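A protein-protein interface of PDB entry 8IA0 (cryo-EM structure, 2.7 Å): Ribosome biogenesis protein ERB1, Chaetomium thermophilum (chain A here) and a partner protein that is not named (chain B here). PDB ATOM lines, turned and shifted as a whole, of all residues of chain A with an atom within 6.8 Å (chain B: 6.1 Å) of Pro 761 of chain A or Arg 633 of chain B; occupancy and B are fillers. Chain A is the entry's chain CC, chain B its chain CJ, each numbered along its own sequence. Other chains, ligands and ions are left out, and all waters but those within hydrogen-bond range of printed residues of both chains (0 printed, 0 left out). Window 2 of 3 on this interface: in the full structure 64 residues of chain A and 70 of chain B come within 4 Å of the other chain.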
ATOM      1  N   PRO A 430     -15.599  16.405  -2.568  1.00  0.00           N
ATOM      2  CA  PRO A 430     -14.491  17.329  -2.835  1.00  0.00           C
ATOM      3  C   PRO A 430     -13.712  17.682  -1.578  1.00  0.00           C
ATOM      4  O   PRO A 430     -14.086  17.279  -0.473  1.00  0.00           O
ATOM      5  CB  PRO A 430     -15.200  18.556  -3.416  1.00  0.00           C
ATOM      6  CG  PRO A 430     -16.534  18.546  -2.764  1.00  0.00           C
ATOM      7  CD  PRO A 430     -16.894  17.103  -2.498  1.00  0.00           C
ATOM      8  N   LEU A 432     -12.364  20.620   0.978  1.00  0.00           N
ATOM      9  CA  LEU A 432     -12.776  21.942   1.412  1.00  0.00           C
ATOM     10  C   LEU A 432     -11.810  22.476   2.457  1.00  0.00           C
ATOM     11  O   LEU A 432     -11.318  21.719   3.300  1.00  0.00           O
ATOM     12  CB  LEU A 432     -14.194  21.914   1.997  1.00  0.00           C
ATOM     13  CG  LEU A 432     -15.340  21.892   0.986  1.00  0.00           C
ATOM     14  CD1 LEU A 432     -16.678  21.895   1.700  1.00  0.00           C
ATOM     15  CD2 LEU A 432     -15.233  23.069   0.034  1.00  0.00           C
ATOM     16  N   PRO A 433     -11.517  23.772   2.421  1.00  0.00           N
ATOM     17  CA  PRO A 433     -10.639  24.362   3.435  1.00  0.00           C
ATOM     18  C   PRO A 433     -11.289  24.332   4.809  1.00  0.00           C
ATOM     19  O   PRO A 433     -12.511  24.362   4.958  1.00  0.00           O
ATOM     20  CB  PRO A 433     -10.434  25.799   2.947  1.00  0.00           C
ATOM     21  CG  PRO A 433     -10.838  25.784   1.506  1.00  0.00           C
ATOM     22  CD  PRO A 433     -11.906  24.749   1.393  1.00  0.00           C
ATOM     23  N   SER A 434     -10.439  24.261   5.827  1.00  0.00           N
ATOM     24  CA  SER A 434     -10.990  24.283   7.175  1.00  0.00           C
ATOM     25  C   SER A 434     -11.562  25.663   7.490  1.00  0.00           C
ATOM     26  O   SER A 434     -11.032  26.675   7.024  1.00  0.00           O
ATOM     27  CB  SER A 434      -9.920  23.928   8.201  1.00  0.00           C
ATOM     28  OG  SER A 434     -10.273  24.400   9.490  1.00  0.00           O
ATOM     29  N   PRO A 435     -12.645  25.721   8.265  1.00  0.00           N
ATOM     30  CA  PRO A 435     -13.236  27.026   8.601  1.00  0.00           C
ATOM     31  C   PRO A 435     -12.299  27.946   9.368  1.00  0.00           C
ATOM     32  O   PRO A 435     -12.508  29.165   9.375  1.00  0.00           O
ATOM     33  CB  PRO A 435     -14.460  26.637   9.440  1.00  0.00           C
ATOM     34  CG  PRO A 435     -14.817  25.281   8.959  1.00  0.00           C
ATOM     35  CD  PRO A 435     -13.505  24.605   8.693  1.00  0.00           C
ATOM     36  N   LEU A 438     -10.809  30.705   7.175  1.00  0.00           N
ATOM     37  CA  LEU A 438     -11.773  31.752   6.839  1.00  0.00           C
ATOM     38  C   LEU A 438     -12.396  32.242   8.142  1.00  0.00           C
ATOM     39  O   LEU A 438     -13.521  31.894   8.507  1.00  0.00           O
ATOM     40  CB  LEU A 438     -12.818  31.216   5.868  1.00  0.00           C
ATOM     41  CG  LEU A 438     -12.343  30.103   4.928  1.00  0.00           C
ATOM     42  CD1 LEU A 438     -13.486  29.582   4.084  1.00  0.00           C
ATOM     43  CD2 LEU A 438     -11.219  30.597   4.026  1.00  0.00           C
ATOM     44  N   MET A 713     -25.740  23.535  -4.575  1.00  0.00           N
ATOM     45  CA  MET A 713     -25.530  23.105  -3.200  1.00  0.00           C
ATOM     46  C   MET A 713     -26.862  22.890  -2.501  1.00  0.00           C
ATOM     47  O   MET A 713     -27.787  23.693  -2.645  1.00  0.00           O
ATOM     48  CB  MET A 713     -24.694  24.126  -2.416  1.00  0.00           C
ATOM     49  CG  MET A 713     -23.466  24.636  -3.151  1.00  0.00           C
ATOM     50  SD  MET A 713     -23.096  26.369  -2.825  1.00  0.00           S
ATOM     51  CE  MET A 713     -24.406  27.182  -3.730  1.00  0.00           C
ATOM     52  N   PHE A 715     -27.961  22.002   1.476  1.00  0.00           N
ATOM     53  CA  PHE A 715     -27.471  21.850   2.841  1.00  0.00           C
ATOM     54  C   PHE A 715     -28.607  21.782   3.853  1.00  0.00           C
ATOM     55  O   PHE A 715     -28.350  21.747   5.061  1.00  0.00           O
ATOM     56  CB  PHE A 715     -26.526  22.997   3.207  1.00  0.00           C
ATOM     57  CG  PHE A 715     -25.134  22.834   2.675  1.00  0.00           C
ATOM     58  CD1 PHE A 715     -24.181  22.139   3.397  1.00  0.00           C
ATOM     59  CD2 PHE A 715     -24.773  23.390   1.463  1.00  0.00           C
ATOM     60  CE1 PHE A 715     -22.899  21.993   2.915  1.00  0.00           C
ATOM     61  CE2 PHE A 715     -23.492  23.248   0.977  1.00  0.00           C
ATOM     62  CZ  PHE A 715     -22.554  22.549   1.704  1.00  0.00           C
ATOM     63  N   GLN A 743     -27.305  28.957   7.405  1.00  0.00           N
ATOM     64  CA  GLN A 743     -26.018  28.483   6.922  1.00  0.00           C
ATOM     65  C   GLN A 743     -25.204  29.658   6.402  1.00  0.00           C
ATOM     66  O   GLN A 743     -25.701  30.462   5.608  1.00  0.00           O
ATOM     67  CB  GLN A 743     -26.196  27.437   5.823  1.00  0.00           C
ATOM     68  CG  GLN A 743     -24.891  26.885   5.282  1.00  0.00           C
ATOM     69  CD  GLN A 743     -24.279  25.833   6.179  1.00  0.00           C
ATOM     70  OE1 GLN A 743     -24.512  24.639   6.004  1.00  0.00           O
ATOM     71  NE2 GLN A 743     -23.479  26.271   7.143  1.00  0.00           N
ATOM     72  N   ILE A 744     -23.957  29.752   6.851  1.00  0.00           N
ATOM     73  CA  ILE A 744     -23.041  30.805   6.434  1.00  0.00           C
ATOM     74  C   ILE A 744     -22.019  30.201   5.484  1.00  0.00           C
ATOM     75  O   ILE A 744     -21.486  29.115   5.740  1.00  0.00           O
ATOM     76  CB  ILE A 744     -22.353  31.458   7.643  1.00  0.00           C
ATOM     77  CG1 ILE A 744     -23.371  31.726   8.752  1.00  0.00           C
ATOM     78  CG2 ILE A 744     -21.667  32.748   7.232  1.00  0.00           C
ATOM     79  CD1 ILE A 744     -24.292  32.892   8.467  1.00  0.00           C
ATOM     80  N   PHE A 745     -21.760  30.893   4.379  1.00  0.00           N
ATOM     81  CA  PHE A 745     -20.791  30.463   3.384  1.00  0.00           C
ATOM     82  C   PHE A 745     -19.684  31.498   3.267  1.00  0.00           C
ATOM     83  O   PHE A 745     -19.819  32.624   3.753  1.00  0.00           O
ATOM     84  CB  PHE A 745     -21.431  30.267   2.009  1.00  0.00           C
ATOM     85  CG  PHE A 745     -22.510  29.228   1.973  1.00  0.00           C
ATOM     86  CD1 PHE A 745     -23.807  29.540   2.328  1.00  0.00           C
ATOM     87  CD2 PHE A 745     -22.228  27.942   1.553  1.00  0.00           C
ATOM     88  CE1 PHE A 745     -24.798  28.587   2.281  1.00  0.00           C
ATOM     89  CE2 PHE A 745     -23.214  26.984   1.506  1.00  0.00           C
ATOM     90  CZ  PHE A 745     -24.501  27.306   1.869  1.00  0.00           C
ATOM     91  N   HIS A 746     -18.591  31.107   2.619  1.00  0.00           N
ATOM     92  CA  HIS A 746     -17.511  32.027   2.285  1.00  0.00           C
ATOM     93  C   HIS A 746     -17.420  32.136   0.769  1.00  0.00           C
ATOM     94  O   HIS A 746     -17.025  31.180   0.093  1.00  0.00           O
ATOM     95  CB  HIS A 746     -16.191  31.549   2.880  1.00  0.00           C
ATOM     96  CG  HIS A 746     -14.982  32.135   2.221  1.00  0.00           C
ATOM     97  ND1 HIS A 746     -14.297  31.487   1.216  1.00  0.00           N
ATOM     98  CD2 HIS A 746     -14.328  33.301   2.431  1.00  0.00           C
ATOM     99  CE1 HIS A 746     -13.278  32.232   0.830  1.00  0.00           C
ATOM    100  NE2 HIS A 746     -13.274  33.338   1.552  1.00  0.00           N
ATOM    101  N   ILE A 759     -16.537  28.901  -3.210  1.00  0.00           N
ATOM    102  CA  ILE A 759     -17.666  28.827  -2.290  1.00  0.00           C
ATOM    103  C   ILE A 759     -17.379  27.731  -1.274  1.00  0.00           C
ATOM    104  O   ILE A 759     -17.290  26.551  -1.634  1.00  0.00           O
ATOM    105  CB  ILE A 759     -18.987  28.552  -3.024  1.00  0.00           C
ATOM    106  CG1 ILE A 759     -19.318  29.695  -3.983  1.00  0.00           C
ATOM    107  CG2 ILE A 759     -20.115  28.354  -2.026  1.00  0.00           C
ATOM    108  CD1 ILE A 759     -18.964  29.407  -5.423  1.00  0.00           C
ATOM    109  N   VAL A 760     -17.232  28.119  -0.010  1.00  0.00           N
ATOM    110  CA  VAL A 760     -16.985  27.170   1.073  1.00  0.00           C
ATOM    111  C   VAL A 760     -17.930  27.473   2.229  1.00  0.00           C
ATOM    112  O   VAL A 760     -17.956  28.609   2.724  1.00  0.00           O
ATOM    113  CB  VAL A 760     -15.523  27.219   1.547  1.00  0.00           C
ATOM    114  CG1 VAL A 760     -15.252  26.093   2.528  1.00  0.00           C
ATOM    115  CG2 VAL A 760     -14.564  27.142   0.369  1.00  0.00           C
ATOM    116  N   PRO A 761     -18.723  26.506   2.687  1.00  0.00           N
ATOM    117  CA  PRO A 761     -19.507  26.720   3.908  1.00  0.00           C
ATOM    118  C   PRO A 761     -18.593  26.817   5.119  1.00  0.00           C
ATOM    119  O   PRO A 761     -17.516  26.218   5.156  1.00  0.00           O
ATOM    120  CB  PRO A 761     -20.403  25.480   3.972  1.00  0.00           C
ATOM    121  CG  PRO A 761     -19.625  24.441   3.241  1.00  0.00           C
ATOM    122  CD  PRO A 761     -18.970  25.175   2.109  1.00  0.00           C
ATOM    123  N   VAL A 762     -19.026  27.582   6.119  1.00  0.00           N
ATOM    124  CA  VAL A 762     -18.194  27.793   7.296  1.00  0.00           C
ATOM    125  C   VAL A 762     -18.925  27.379   8.568  1.00  0.00           C
ATOM    126  O   VAL A 762     -18.368  26.659   9.402  1.00  0.00           O
ATOM    127  CB  VAL A 762     -17.717  29.256   7.386  1.00  0.00           C
ATOM    128  CG1 VAL A 762     -16.544  29.482   6.448  1.00  0.00           C
ATOM    129  CG2 VAL A 762     -18.843  30.217   7.060  1.00  0.00           C
ATOM    130  N   LYS A 763     -20.171  27.819   8.730  1.00  0.00           N
ATOM    131  CA  LYS A 763     -20.853  27.625  10.003  1.00  0.00           C
ATOM    132  C   LYS A 763     -22.349  27.474   9.782  1.00  0.00           C
ATOM    133  O   LYS A 763     -22.941  28.214   8.991  1.00  0.00           O
ATOM    134  CB  LYS A 763     -20.579  28.800  10.949  1.00  0.00           C
ATOM    135  CG  LYS A 763     -21.069  28.588  12.370  1.00  0.00           C
ATOM    136  CD  LYS A 763     -19.999  27.943  13.232  1.00  0.00           C
ATOM    137  CE  LYS A 763     -20.580  26.844  14.100  1.00  0.00           C
ATOM    138  NZ  LYS A 763     -21.510  27.391  15.121  1.00  0.00           N
ATOM    139  N   ALA B 628     -18.031  13.952  11.366  1.00  0.00           N
ATOM    140  CA  ALA B 628     -19.380  14.057  10.823  1.00  0.00           C
ATOM    141  C   ALA B 628     -19.622  15.422  10.191  1.00  0.00           C
ATOM    142  O   ALA B 628     -20.210  15.516   9.108  1.00  0.00           O
ATOM    143  CB  ALA B 628     -20.410  13.784  11.918  1.00  0.00           C
ATOM    144  N   GLU B 629     -19.182  16.493  10.856  1.00  0.00           N
ATOM    145  CA  GLU B 629     -19.379  17.834  10.316  1.00  0.00           C
ATOM    146  C   GLU B 629     -18.610  18.022   9.013  1.00  0.00           C
ATOM    147  O   GLU B 629     -19.117  18.628   8.062  1.00  0.00           O
ATOM    148  CB  GLU B 629     -18.967  18.883  11.347  1.00  0.00           C
ATOM    149  CG  GLU B 629     -20.133  19.574  12.049  1.00  0.00           C
ATOM    150  CD  GLU B 629     -21.050  18.615  12.787  1.00  0.00           C
ATOM    151  OE1 GLU B 629     -20.578  17.550  13.235  1.00  0.00           O
ATOM    152  OE2 GLU B 629     -22.251  18.932  12.920  1.00  0.00           O
ATOM    153  N   GLU B 630     -17.378  17.516   8.956  1.00  0.00           N
ATOM    154  CA  GLU B 630     -16.625  17.562   7.707  1.00  0.00           C
ATOM    155  C   GLU B 630     -17.315  16.741   6.626  1.00  0.00           C
ATOM    156  O   GLU B 630     -17.323  17.127   5.451  1.00  0.00           O
ATOM    157  CB  GLU B 630     -15.197  17.070   7.934  1.00  0.00           C
ATOM    158  CG  GLU B 630     -14.325  17.111   6.692  1.00  0.00           C
ATOM    159  CD  GLU B 630     -14.054  18.525   6.216  1.00  0.00           C
ATOM    160  OE1 GLU B 630     -14.039  19.447   7.059  1.00  0.00           O
ATOM    161  OE2 GLU B 630     -13.857  18.716   4.998  1.00  0.00           O
ATOM    162  N   LEU B 631     -17.898  15.603   7.005  1.00  0.00           N
ATOM    163  CA  LEU B 631     -18.653  14.800   6.051  1.00  0.00           C
ATOM    164  C   LEU B 631     -19.857  15.568   5.522  1.00  0.00           C
ATOM    165  O   LEU B 631     -20.142  15.540   4.320  1.00  0.00           O
ATOM    166  CB  LEU B 631     -19.095  13.493   6.715  1.00  0.00           C
ATOM    167  CG  LEU B 631     -19.523  12.297   5.860  1.00  0.00           C
ATOM    168  CD1 LEU B 631     -20.986  12.370   5.456  1.00  0.00           C
ATOM    169  CD2 LEU B 631     -18.634  12.179   4.642  1.00  0.00           C
ATOM    170  N   GLU B 632     -20.574  16.263   6.407  1.00  0.00           N
ATOM    171  CA  GLU B 632     -21.755  17.010   5.986  1.00  0.00           C
ATOM    172  C   GLU B 632     -21.384  18.172   5.074  1.00  0.00           C
ATOM    173  O   GLU B 632     -22.088  18.451   4.096  1.00  0.00           O
ATOM    174  CB  GLU B 632     -22.518  17.517   7.210  1.00  0.00           C
ATOM    175  CG  GLU B 632     -23.236  16.444   8.028  1.00  0.00           C
ATOM    176  CD  GLU B 632     -23.724  15.270   7.198  1.00  0.00           C
ATOM    177  OE1 GLU B 632     -22.938  14.328   6.968  1.00  0.00           O
ATOM    178  OE2 GLU B 632     -24.898  15.289   6.773  1.00  0.00           O
ATOM    179  N   ARG B 633     -20.291  18.871   5.384  1.00  0.00           N
ATOM    180  CA  ARG B 633     -19.910  20.049   4.607  1.00  0.00           C
ATOM    181  C   ARG B 633     -19.585  19.681   3.164  1.00  0.00           C
ATOM    182  O   ARG B 633     -19.986  20.381   2.228  1.00  0.00           O
ATOM    183  CB  ARG B 633     -18.720  20.745   5.262  1.00  0.00           C
ATOM    184  CG  ARG B 633     -19.074  21.602   6.460  1.00  0.00           C
ATOM    185  CD  ARG B 633     -17.835  21.927   7.269  1.00  0.00           C
ATOM    186  NE  ARG B 633     -17.031  22.956   6.625  1.00  0.00           N
ATOM    187  CZ  ARG B 633     -15.779  22.786   6.227  1.00  0.00           C
ATOM    188  NH1 ARG B 633     -15.152  21.632   6.391  1.00  0.00           N
ATOM    189  NH2 ARG B 633     -15.139  23.796   5.648  1.00  0.00           N
ATOM    190  N   ALA B 634     -18.849  18.586   2.967  1.00  0.00           N
ATOM    191  CA  ALA B 634     -18.479  18.185   1.614  1.00  0.00           C
ATOM    192  C   ALA B 634     -19.665  17.587   0.868  1.00  0.00           C
ATOM    193  O   ALA B 634     -19.808  17.787  -0.344  1.00  0.00           O
ATOM    194  CB  ALA B 634     -17.320  17.193   1.659  1.00  0.00           C
ATOM    195  N   LYS B 635     -20.522  16.850   1.573  1.00  0.00           N
ATOM    196  CA  LYS B 635     -21.658  16.207   0.922  1.00  0.00           C
ATOM    197  C   LYS B 635     -22.649  17.234   0.391  1.00  0.00           C
ATOM    198  O   LYS B 635     -23.338  16.986  -0.605  1.00  0.00           O
ATOM    199  CB  LYS B 635     -22.340  15.249   1.896  1.00  0.00           C
ATOM    200  CG  LYS B 635     -23.118  14.134   1.229  1.00  0.00           C
ATOM    201  CD  LYS B 635     -24.444  13.899   1.925  1.00  0.00           C
ATOM    202  CE  LYS B 635     -24.232  13.465   3.364  1.00  0.00           C
ATOM    203  NZ  LYS B 635     -25.514  13.390   4.114  1.00  0.00           N
ATOM    204  N   GLY B 636     -22.735  18.394   1.042  1.00  0.00           N
ATOM    205  CA  GLY B 636     -23.656  19.418   0.581  1.00  0.00           C
ATOM    206  C   GLY B 636     -23.178  20.109  -0.681  1.00  0.00           C
ATOM    207  O   GLY B 636     -23.967  20.729  -1.396  1.00  0.00           O
ATOM    208  N   MET B 637     -21.881  20.008  -0.972  1.00  0.00           N
ATOM    209  CA  MET B 637     -21.333  20.642  -2.163  1.00  0.00           C
ATOM    210  C   MET B 637     -21.518  19.786  -3.410  1.00  0.00           C
ATOM    211  O   MET B 637     -21.195  20.240  -4.511  1.00  0.00           O
ATOM    212  CB  MET B 637     -19.850  20.945  -1.954  1.00  0.00           C
ATOM    213  CG  MET B 637     -19.575  22.173  -1.099  1.00  0.00           C
ATOM    214  SD  MET B 637     -20.400  23.667  -1.673  1.00  0.00           S
ATOM    215  CE  MET B 637     -19.282  24.188  -2.967  1.00  0.00           C
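O of Pro 433 of chain A is in hydrogen-bond range of NH2 of Arg 633 of chain B. The guanidinium group (NH2) of Arg 633 of chain B sits at hydrogen-bond distance from the backbone carbonyl oxygen (O) of Pro 761 of chain A.
OE2 of Glu 632 of chain B is in salt-bridge range of NZ of Lys 635 of chain B (3.3 Å). The guanidinium group (NH1) of Arg 633 of chain B lies within salt-bridge range of the side-chain carboxylate (OE1) of Glu 630 of chain B, 2.5 Å away. The backbone carbonyl oxygen of Val 760 of chain A sits at hydrogen-bond distance from the backbone NH of His 746 of chain A (2.6 Å).
Pro 430 of chain A touches Ala 634 of chain B. Arg 633 of chain B touches Leu 432 of chain A. Met 713 of chain A touches Gly 636 of chain B (CA to O, 3.4 Å). Met 713 of chain A touches Met 637 of chain B (CG to SD, 3.5 Å). Phe 715 of chain A touches Glu 632 of chain B (CE1 to O, 3.8 Å). Phe 715 of chain A touches Arg 633 of chain B (CE1 to O, 3.4 Å). CZ of Phe 715 of chain A touches C of Gly 636 of chain B, 3.5 Å away. Met 637 of chain B touches Phe 715 of chain A (N to CZ, 3.8 Å). Ile 759 of chain A touches Met 637 of chain B (O to CE, 3.4 Å). Val 760 of chain A touches Arg 633 of chain B (CG1 to NH2, 3.9 Å).
Of the printed residues of chain B, Leu 432 of chain A touches Arg 633. Printed residues of chain B within 4 Å of Pro 433 of chain A: Arg 633. Printed residues of chain B within 4 Å of Met 713 of chain A: Gly 636 (3.4 Å) and Met 637 (3.5 Å). Pro 761 of chain A touches one residue of chain B. Ala 628 of chain B touches none of the printed residues of chain A. Of the printed residues of chain A, Glu 632 of chain B touches Phe 715 (3.8 Å). Arg 633 of chain B touches just these residues of chain A: Leu 432 (3.7 Å), Pro 433 (2.8 Å), Pro 435 (3.5 Å), Phe 715 (3.4 Å), Val 760 (3.9 Å) and Pro 761 (3.4 Å). Printed residues of chain A within 4 Å of Met 637 of chain B: Met 713, Phe 715 and Ile 759. The nearest residue of chain A that does not touch Arg 633 of chain B is Ser 434 of chain A (4.4 Å).
Along chain A the printed residues that touch a printed residue of chain B span positions 430 to 761. Hydrophobic or aromatic side chains of chain B that line the printed part of chain A: Ala 634 and Met 637. Among the printed residues, 13 pairs touch across the chains.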
